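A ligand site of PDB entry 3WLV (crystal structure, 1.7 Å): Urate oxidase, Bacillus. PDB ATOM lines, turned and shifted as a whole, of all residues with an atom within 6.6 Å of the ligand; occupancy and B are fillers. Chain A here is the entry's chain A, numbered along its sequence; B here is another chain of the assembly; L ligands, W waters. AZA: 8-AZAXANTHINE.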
ATOM      1  N   SER A 176       7.296 -22.250 -31.275  1.00  0.00           N
ATOM      2  CA  SER A 176       8.235 -21.224 -31.721  1.00  0.00           C
ATOM      3  C   SER A 176       7.837 -19.851 -31.193  1.00  0.00           C
ATOM      4  O   SER A 176       6.678 -19.613 -30.803  1.00  0.00           O
ATOM      5  CB  SER A 176       8.347 -21.197 -33.270  1.00  0.00           C
ATOM      6  OG  SER A 176       7.275 -20.494 -33.858  1.00  0.00           O
ATOM      7  N   PHE A 177       8.815 -18.962 -31.140  1.00  0.00           N
ATOM      8  CA  PHE A 177       8.563 -17.537 -30.966  1.00  0.00           C
ATOM      9  C   PHE A 177       9.566 -16.763 -31.823  1.00  0.00           C
ATOM     10  O   PHE A 177      10.723 -16.601 -31.436  1.00  0.00           O
ATOM     11  CB  PHE A 177       8.652 -17.106 -29.510  1.00  0.00           C
ATOM     12  CG  PHE A 177       8.131 -15.705 -29.284  1.00  0.00           C
ATOM     13  CD1 PHE A 177       6.816 -15.391 -29.597  1.00  0.00           C
ATOM     14  CD2 PHE A 177       8.956 -14.718 -28.751  1.00  0.00           C
ATOM     15  CE1 PHE A 177       6.343 -14.092 -29.404  1.00  0.00           C
ATOM     16  CE2 PHE A 177       8.481 -13.453 -28.543  1.00  0.00           C
ATOM     17  CZ  PHE A 177       7.177 -13.119 -28.875  1.00  0.00           C
ATOM     18  N   PHE A 180       9.089 -11.208 -33.856  1.00  0.00           N
ATOM     19  CA  PHE A 180       8.750 -10.097 -32.988  1.00  0.00           C
ATOM     20  C   PHE A 180       9.669  -8.892 -33.241  1.00  0.00           C
ATOM     21  O   PHE A 180      10.683  -8.993 -33.953  1.00  0.00           O
ATOM     22  CB  PHE A 180       8.796 -10.524 -31.518  1.00  0.00           C
ATOM     23  CG  PHE A 180      10.065 -11.221 -31.102  1.00  0.00           C
ATOM     24  CD1 PHE A 180      11.137 -10.496 -30.626  1.00  0.00           C
ATOM     25  CD2 PHE A 180      10.187 -12.608 -31.184  1.00  0.00           C
ATOM     26  CE1 PHE A 180      12.296 -11.134 -30.248  1.00  0.00           C
ATOM     27  CE2 PHE A 180      11.363 -13.243 -30.800  1.00  0.00           C
ATOM     28  CZ  PHE A 180      12.416 -12.493 -30.334  1.00  0.00           C
ATOM     29  N   LEU A 188      16.307 -10.704 -26.839  1.00  0.00           N
ATOM     30  CA  LEU A 188      15.798 -12.074 -26.921  1.00  0.00           C
ATOM     31  C   LEU A 188      16.060 -12.695 -28.302  1.00  0.00           C
ATOM     32  O   LEU A 188      15.596 -12.182 -29.307  1.00  0.00           O
ATOM     33  CB  LEU A 188      14.285 -12.108 -26.648  1.00  0.00           C
ATOM     34  CG  LEU A 188      13.578 -13.468 -26.664  1.00  0.00           C
ATOM     35  CD1 LEU A 188      13.992 -14.309 -25.458  1.00  0.00           C
ATOM     36  CD2 LEU A 188      12.058 -13.237 -26.673  1.00  0.00           C
ATOM     37  N   ARG A 194      11.256 -24.115 -28.755  1.00  0.00           N
ATOM     38  CA  ARG A 194      11.425 -23.909 -27.317  1.00  0.00           C
ATOM     39  C   ARG A 194      10.502 -24.852 -26.549  1.00  0.00           C
ATOM     40  O   ARG A 194       9.461 -25.268 -27.078  1.00  0.00           O
ATOM     41  CB  ARG A 194      11.091 -22.446 -26.962  1.00  0.00           C
ATOM     42  CG  ARG A 194       9.661 -22.057 -27.251  1.00  0.00           C
ATOM     43  CD  ARG A 194       9.380 -20.583 -26.890  1.00  0.00           C
ATOM     44  NE  ARG A 194       7.980 -20.219 -27.100  1.00  0.00           N
ATOM     45  CZ  ARG A 194       7.465 -19.056 -26.717  1.00  0.00           C
ATOM     46  NH1 ARG A 194       8.267 -18.158 -26.145  1.00  0.00           N
ATOM     47  NH2 ARG A 194       6.193 -18.784 -26.931  1.00  0.00           N
ATOM     48  N   LEU A 196       8.035 -24.627 -24.338  1.00  0.00           N
ATOM     49  CA  LEU A 196       7.133 -23.633 -23.790  1.00  0.00           C
ATOM     50  C   LEU A 196       6.460 -24.121 -22.514  1.00  0.00           C
ATOM     51  O   LEU A 196       5.877 -25.177 -22.501  1.00  0.00           O
ATOM     52  CB  LEU A 196       6.078 -23.284 -24.835  1.00  0.00           C
ATOM     53  CG  LEU A 196       5.008 -22.335 -24.337  1.00  0.00           C
ATOM     54  CD1 LEU A 196       5.611 -21.008 -23.888  1.00  0.00           C
ATOM     55  CD2 LEU A 196       4.019 -22.105 -25.460  1.00  0.00           C
ATOM     56  N   LEU A 240       2.912 -20.614 -31.918  1.00  0.00           N
ATOM     57  CA  LEU A 240       3.679 -19.505 -32.476  1.00  0.00           C
ATOM     58  C   LEU A 240       3.925 -18.400 -31.430  1.00  0.00           C
ATOM     59  O   LEU A 240       4.659 -17.444 -31.697  1.00  0.00           O
ATOM     60  CB  LEU A 240       2.915 -18.941 -33.671  1.00  0.00           C
ATOM     61  CG  LEU A 240       2.737 -19.928 -34.835  1.00  0.00           C
ATOM     62  CD1 LEU A 240       1.810 -19.333 -35.862  1.00  0.00           C
ATOM     63  CD2 LEU A 240       4.073 -20.278 -35.477  1.00  0.00           C
ATOM     64  N   SER A 241       3.264 -18.561 -30.286  1.00  0.00           N
ATOM     65  CA  SER A 241       3.363 -17.732 -29.093  1.00  0.00           C
ATOM     66  C   SER A 241       2.331 -18.271 -28.107  1.00  0.00           C
ATOM     67  O   SER A 241       1.491 -19.101 -28.456  1.00  0.00           O
ATOM     68  CB  SER A 241       2.998 -16.289 -29.417  1.00  0.00           C
ATOM     69  OG  SER A 241       1.654 -16.210 -29.835  1.00  0.00           O
ATOM     70  N   ILE A 242       2.357 -17.793 -26.885  1.00  0.00           N
ATOM     71  CA  ILE A 242       1.337 -18.132 -25.905  1.00  0.00           C
ATOM     72  C   ILE A 242      -0.012 -17.519 -26.330  1.00  0.00           C
ATOM     73  O   ILE A 242      -1.064 -18.167 -26.233  1.00  0.00           O
ATOM     74  CB  ILE A 242       1.714 -17.654 -24.509  1.00  0.00           C
ATOM     75  CG1 ILE A 242       2.993 -18.374 -24.044  1.00  0.00           C
ATOM     76  CG2 ILE A 242       0.566 -17.899 -23.508  1.00  0.00           C
ATOM     77  CD1 ILE A 242       3.574 -17.814 -22.724  1.00  0.00           C
ATOM     78  N   GLN A 243       0.055 -16.284 -26.831  1.00  0.00           N
ATOM     79  CA  GLN A 243      -1.115 -15.581 -27.369  1.00  0.00           C
ATOM     80  C   GLN A 243      -1.866 -16.457 -28.380  1.00  0.00           C
ATOM     81  O   GLN A 243      -3.096 -16.619 -28.308  1.00  0.00           O
ATOM     82  CB  GLN A 243      -0.699 -14.272 -28.037  1.00  0.00           C
ATOM     83  CG  GLN A 243      -0.168 -13.160 -27.087  1.00  0.00           C
ATOM     84  CD  GLN A 243       1.321 -13.182 -26.865  1.00  0.00           C
ATOM     85  OE1 GLN A 243       1.925 -14.259 -26.698  1.00  0.00           O
ATOM     86  NE2 GLN A 243       1.945 -12.003 -26.822  1.00  0.00           N
ATOM     87  N   ASN A 269       4.232 -17.028 -18.691  1.00  0.00           N
ATOM     88  CA  ASN A 269       5.336 -17.720 -19.325  1.00  0.00           C
ATOM     89  C   ASN A 269       6.430 -17.978 -18.313  1.00  0.00           C
ATOM     90  O   ASN A 269       7.020 -17.031 -17.749  1.00  0.00           O
ATOM     91  CB  ASN A 269       5.849 -16.903 -20.509  1.00  0.00           C
ATOM     92  CG  ASN A 269       6.837 -17.673 -21.379  1.00  0.00           C
ATOM     93  OD1 ASN A 269       7.356 -18.730 -21.001  1.00  0.00           O
ATOM     94  ND2 ASN A 269       7.147 -17.099 -22.514  1.00  0.00           N
ATOM     95  N   GLY A 295       6.520 -13.313 -18.318  1.00  0.00           N
ATOM     96  CA  GLY A 295       5.549 -12.743 -19.232  1.00  0.00           C
ATOM     97  C   GLY A 295       4.160 -13.201 -18.872  1.00  0.00           C
ATOM     98  O   GLY A 295       3.973 -14.242 -18.232  1.00  0.00           O
ATOM     99  N   PHE A 296       3.156 -12.428 -19.275  1.00  0.00           N
ATOM    100  CA  PHE A 296       1.786 -12.841 -19.083  1.00  0.00           C
ATOM    101  C   PHE A 296       0.925 -12.304 -20.207  1.00  0.00           C
ATOM    102  O   PHE A 296       1.272 -11.326 -20.860  1.00  0.00           O
ATOM    103  CB  PHE A 296       1.262 -12.404 -17.724  1.00  0.00           C
ATOM    104  CG  PHE A 296       1.219 -10.920 -17.530  1.00  0.00           C
ATOM    105  CD1 PHE A 296       0.171 -10.153 -18.015  1.00  0.00           C
ATOM    106  CD2 PHE A 296       2.245 -10.274 -16.854  1.00  0.00           C
ATOM    107  CE1 PHE A 296       0.114  -8.775 -17.803  1.00  0.00           C
ATOM    108  CE2 PHE A 296       2.214  -8.925 -16.656  1.00  0.00           C
ATOM    109  CZ  PHE A 296       1.158  -8.157 -17.135  1.00  0.00           C
ATOM    110  N   GLN A 297      -0.214 -12.964 -20.412  1.00  0.00           N
ATOM    111  CA  GLN A 297      -1.149 -12.615 -21.461  1.00  0.00           C
ATOM    112  C   GLN A 297      -2.569 -12.734 -20.875  1.00  0.00           C
ATOM    113  O   GLN A 297      -2.814 -13.549 -19.990  1.00  0.00           O
ATOM    114  CB  GLN A 297      -1.027 -13.571 -22.648  1.00  0.00           C
ATOM    115  CG  GLN A 297       0.316 -13.639 -23.324  1.00  0.00           C
ATOM    116  CD  GLN A 297       1.444 -14.281 -22.550  1.00  0.00           C
ATOM    117  OE1 GLN A 297       1.262 -15.167 -21.696  1.00  0.00           O
ATOM    118  NE2 GLN A 297       2.650 -13.851 -22.875  1.00  0.00           N
ATOM    119  N   TYR B   4      -1.092  -7.885 -22.626  1.00  0.00           N
ATOM    120  CA  TYR B   4       0.010  -8.785 -22.270  1.00  0.00           C
ATOM    121  C   TYR B   4       1.139  -7.943 -21.680  1.00  0.00           C
ATOM    122  O   TYR B   4       1.106  -6.721 -21.762  1.00  0.00           O
ATOM    123  CB  TYR B   4       0.469  -9.624 -23.483  1.00  0.00           C
ATOM    124  CG  TYR B   4       1.373  -8.879 -24.466  1.00  0.00           C
ATOM    125  CD1 TYR B   4       0.904  -7.802 -25.177  1.00  0.00           C
ATOM    126  CD2 TYR B   4       2.689  -9.283 -24.660  1.00  0.00           C
ATOM    127  CE1 TYR B   4       1.729  -7.110 -26.080  1.00  0.00           C
ATOM    128  CE2 TYR B   4       3.524  -8.628 -25.529  1.00  0.00           C
ATOM    129  CZ  TYR B   4       3.050  -7.530 -26.231  1.00  0.00           C
ATOM    130  OH  TYR B   4       3.880  -6.867 -27.090  1.00  0.00           O
ATOM    131  N   GLY B   5       2.095  -8.583 -21.031  1.00  0.00           N
ATOM    132  CA  GLY B   5       3.114  -7.822 -20.351  1.00  0.00           C
ATOM    133  C   GLY B   5       4.094  -8.649 -19.557  1.00  0.00           C
ATOM    134  O   GLY B   5       4.249  -9.823 -19.845  1.00  0.00           O
ATOM    135  N   LYS B   6       4.731  -8.027 -18.582  1.00  0.00           N
ATOM    136  CA  LYS B   6       5.776  -8.658 -17.787  1.00  0.00           C
ATOM    137  C   LYS B   6       5.544  -8.319 -16.337  1.00  0.00           C
ATOM    138  O   LYS B   6       5.272  -7.171 -16.025  1.00  0.00           O
ATOM    139  CB  LYS B   6       7.170  -8.148 -18.195  1.00  0.00           C
ATOM    140  CG  LYS B   6       8.323  -9.081 -17.781  1.00  0.00           C
ATOM    141  CD  LYS B   6       8.426 -10.256 -18.761  1.00  0.00           C
ATOM    142  CE  LYS B   6       9.675 -11.046 -18.689  1.00  0.00           C
ATOM    143  NZ  LYS B   6       9.719 -12.069 -19.793  1.00  0.00           N
ATOM    144  N   ASN B  60       3.523 -12.125 -35.049  1.00  0.00           N
ATOM    145  CA  ASN B  60       4.293 -11.420 -34.040  1.00  0.00           C
ATOM    146  C   ASN B  60       4.887 -10.104 -34.503  1.00  0.00           C
ATOM    147  O   ASN B  60       5.622  -9.460 -33.756  1.00  0.00           O
ATOM    148  CB  ASN B  60       5.371 -12.339 -33.472  1.00  0.00           C
ATOM    149  CG  ASN B  60       4.784 -13.483 -32.704  1.00  0.00           C
ATOM    150  OD1 ASN B  60       3.795 -13.317 -31.994  1.00  0.00           O
ATOM    151  ND2 ASN B  60       5.365 -14.670 -32.850  1.00  0.00           N
ATOM    152  N   VAL B  63       4.494  -7.356 -32.053  1.00  0.00           N
ATOM    153  CA  VAL B  63       4.702  -7.756 -30.682  1.00  0.00           C
ATOM    154  C   VAL B  63       6.044  -7.232 -30.178  1.00  0.00           C
ATOM    155  O   VAL B  63       7.091  -7.620 -30.692  1.00  0.00           O
ATOM    156  CB  VAL B  63       4.686  -9.307 -30.519  1.00  0.00           C
ATOM    157  CG1 VAL B  63       5.074  -9.704 -29.099  1.00  0.00           C
ATOM    158  CG2 VAL B  63       3.307  -9.846 -30.829  1.00  0.00           C
ATOM    159  N   VAL B  64       5.998  -6.372 -29.177  1.00  0.00           N
ATOM    160  CA  VAL B  64       7.173  -6.090 -28.345  1.00  0.00           C
ATOM    161  C   VAL B  64       7.321  -7.288 -27.408  1.00  0.00           C
ATOM    162  O   VAL B  64       6.388  -7.613 -26.656  1.00  0.00           O
ATOM    163  CB  VAL B  64       6.984  -4.822 -27.493  1.00  0.00           C
ATOM    164  CG1 VAL B  64       8.199  -4.536 -26.655  1.00  0.00           C
ATOM    165  CG2 VAL B  64       6.673  -3.643 -28.383  1.00  0.00           C
ATOM    166  N   ALA B  65       8.461  -7.962 -27.444  1.00  0.00           N
ATOM    167  CA  ALA B  65       8.676  -9.113 -26.571  1.00  0.00           C
ATOM    168  C   ALA B  65       8.605  -8.671 -25.118  1.00  0.00           C
ATOM    169  O   ALA B  65       9.032  -7.576 -24.778  1.00  0.00           O
ATOM    170  CB  ALA B  65       9.998  -9.794 -26.871  1.00  0.00           C
ATOM    171  N   THR B  66       8.001  -9.486 -24.279  1.00  0.00           N
ATOM    172  CA  THR B  66       7.904  -9.138 -22.880  1.00  0.00           C
ATOM    173  C   THR B  66       9.306  -8.991 -22.279  1.00  0.00           C
ATOM    174  O   THR B  66       9.521  -8.166 -21.409  1.00  0.00           O
ATOM    175  CB  THR B  66       7.047 -10.154 -22.102  1.00  0.00           C
ATOM    176  OG1 THR B  66       7.725 -11.418 -22.052  1.00  0.00           O
ATOM    177  CG2 THR B  66       5.661 -10.292 -22.751  1.00  0.00           C
ATOM    178  N   ASP B  67      10.247  -9.769 -22.777  1.00  0.00           N
ATOM    179  CA  ASP B  67      11.648  -9.651 -22.352  1.00  0.00           C
ATOM    180  C   ASP B  67      12.187  -8.265 -22.684  1.00  0.00           C
ATOM    181  O   ASP B  67      12.959  -7.689 -21.916  1.00  0.00           O
ATOM    182  CB  ASP B  67      12.497 -10.696 -23.063  1.00  0.00           C
ATOM    183  CG  ASP B  67      13.935 -10.716 -22.563  1.00  0.00           C
ATOM    184  OD1 ASP B  67      14.188 -11.330 -21.509  1.00  0.00           O
ATOM    185  OD2 ASP B  67      14.822 -10.134 -23.230  1.00  0.00           O
ATOM    186  N   SER B  68      11.775  -7.716 -23.826  1.00  0.00           N
ATOM    187  CA  SER B  68      12.148  -6.351 -24.188  1.00  0.00           C
ATOM    188  C   SER B  68      11.556  -5.313 -23.262  1.00  0.00           C
ATOM    189  O   SER B  68      12.188  -4.290 -22.974  1.00  0.00           O
ATOM    190  CB  SER B  68      11.775  -6.057 -25.636  1.00  0.00           C
ATOM    191  OG  SER B  68      12.339  -7.044 -26.480  1.00  0.00           O
ATOM    192  N   MET B  69      10.341  -5.562 -22.796  1.00  0.00           N
ATOM    193  CA  MET B  69       9.712  -4.658 -21.832  1.00  0.00           C
ATOM    194  C   MET B  69      10.507  -4.616 -20.541  1.00  0.00           C
ATOM    195  O   MET B  69      10.680  -3.559 -19.914  1.00  0.00           O
ATOM    196  CB  MET B  69       8.265  -5.087 -21.558  1.00  0.00           C
ATOM    197  CG  MET B  69       7.345  -5.033 -22.752  1.00  0.00           C
ATOM    198  SD  MET B  69       5.733  -5.717 -22.252  1.00  0.00           S
ATOM    199  CE  MET B  69       4.945  -5.942 -23.882  1.00  0.00           C
HETATM  200  N1  AZA L   1       4.740 -14.269 -26.068  1.00  0.00           N
HETATM  201  C2  AZA L   1       5.390 -15.468 -26.061  1.00  0.00           C
HETATM  202  O2  AZA L   1       4.765 -16.486 -26.303  1.00  0.00           O
HETATM  203  N3  AZA L   1       6.704 -15.515 -25.774  1.00  0.00           N
HETATM  204  C4  AZA L   1       7.407 -14.384 -25.527  1.00  0.00           C
HETATM  205  C5  AZA L   1       6.740 -13.172 -25.543  1.00  0.00           C
HETATM  206  C6  AZA L   1       5.376 -13.165 -25.831  1.00  0.00           C
HETATM  207  O6  AZA L   1       4.760 -12.108 -25.856  1.00  0.00           O
HETATM  208  N7  AZA L   1       7.611 -12.227 -25.260  1.00  0.00           N
HETATM  209  N8  AZA L   1       8.802 -12.775 -25.049  1.00  0.00           N
HETATM  210  N9  AZA L   1       8.709 -14.124 -25.179  1.00  0.00           N
HETATM  211  O   HOH W   1      10.391 -13.190 -22.574  1.00  0.00           O
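The backbone NH (N) of Gln 243 lies close to the side-chain hydroxyl (OG) of Ser 241 (3.4 Å).
NZ of Lys 6 of chain B lies within hydrogen-bond range of OG1 of Thr 66 of chain B (3.1 Å).
The backbone carbonyl oxygen of Gly 295 lies within hydrogen-bond range of the backbone NH of Asn 269 (2.8 Å).
The side-chain hydroxyl of Tyr 4 of chain B is in hydrogen-bond range of the backbone carbonyl oxygen of Val 64 of chain B, at 2.7 Å.
An oxygen (O2) of the ligand sits at hydrogen-bond distance from the guanidinium group (NH2) of Arg 194 (2.8 Å).
N of Ile 242 is in hydrogen-bond range of O2 of the ligand, 2.8 Å away.
A nitrogen (N1) of the ligand sits at hydrogen-bond distance from the side-chain amide oxygen (OE1) of Gln 243 (2.9 Å).
N of Thr 66 of chain B sits at hydrogen-bond distance from N7 of the ligand (2.9 Å).
A nitrogen (N7) of the ligand is in hydrogen-bond range of the side-chain hydroxyl (OG1) of Thr 66 of chain B (3.3 Å).
Phe 177 touches the ligand.
Leu 188 touches the ligand (CD2 to N8, 3.7 Å).
Ser 241 touches the ligand.
Asn 269 touches the ligand.
Gln 297 touches the ligand (NE2 to N1, 3.8 Å).
CD2 of Tyr 4 of chain B touches O6 of the ligand, 3.7 Å away.
Ala 65 of chain B touches the ligand.
Hydrophobic or aromatic side chains that line the ligand: Phe 177, Leu 188, Ile 242, Tyr 4 of chain B and Ala 65 of chain B.
Water W1 lies within hydrogen-bond range of a nitrogen (N8) of the ligand (3.0 Å), the side-chain amino group of Lys 6 of chain B (3.1 Å), the side-chain hydroxyl of Thr 66 of chain B (3.2 Å) and the backbone NH of Asp 67 of chain B (3.4 Å).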
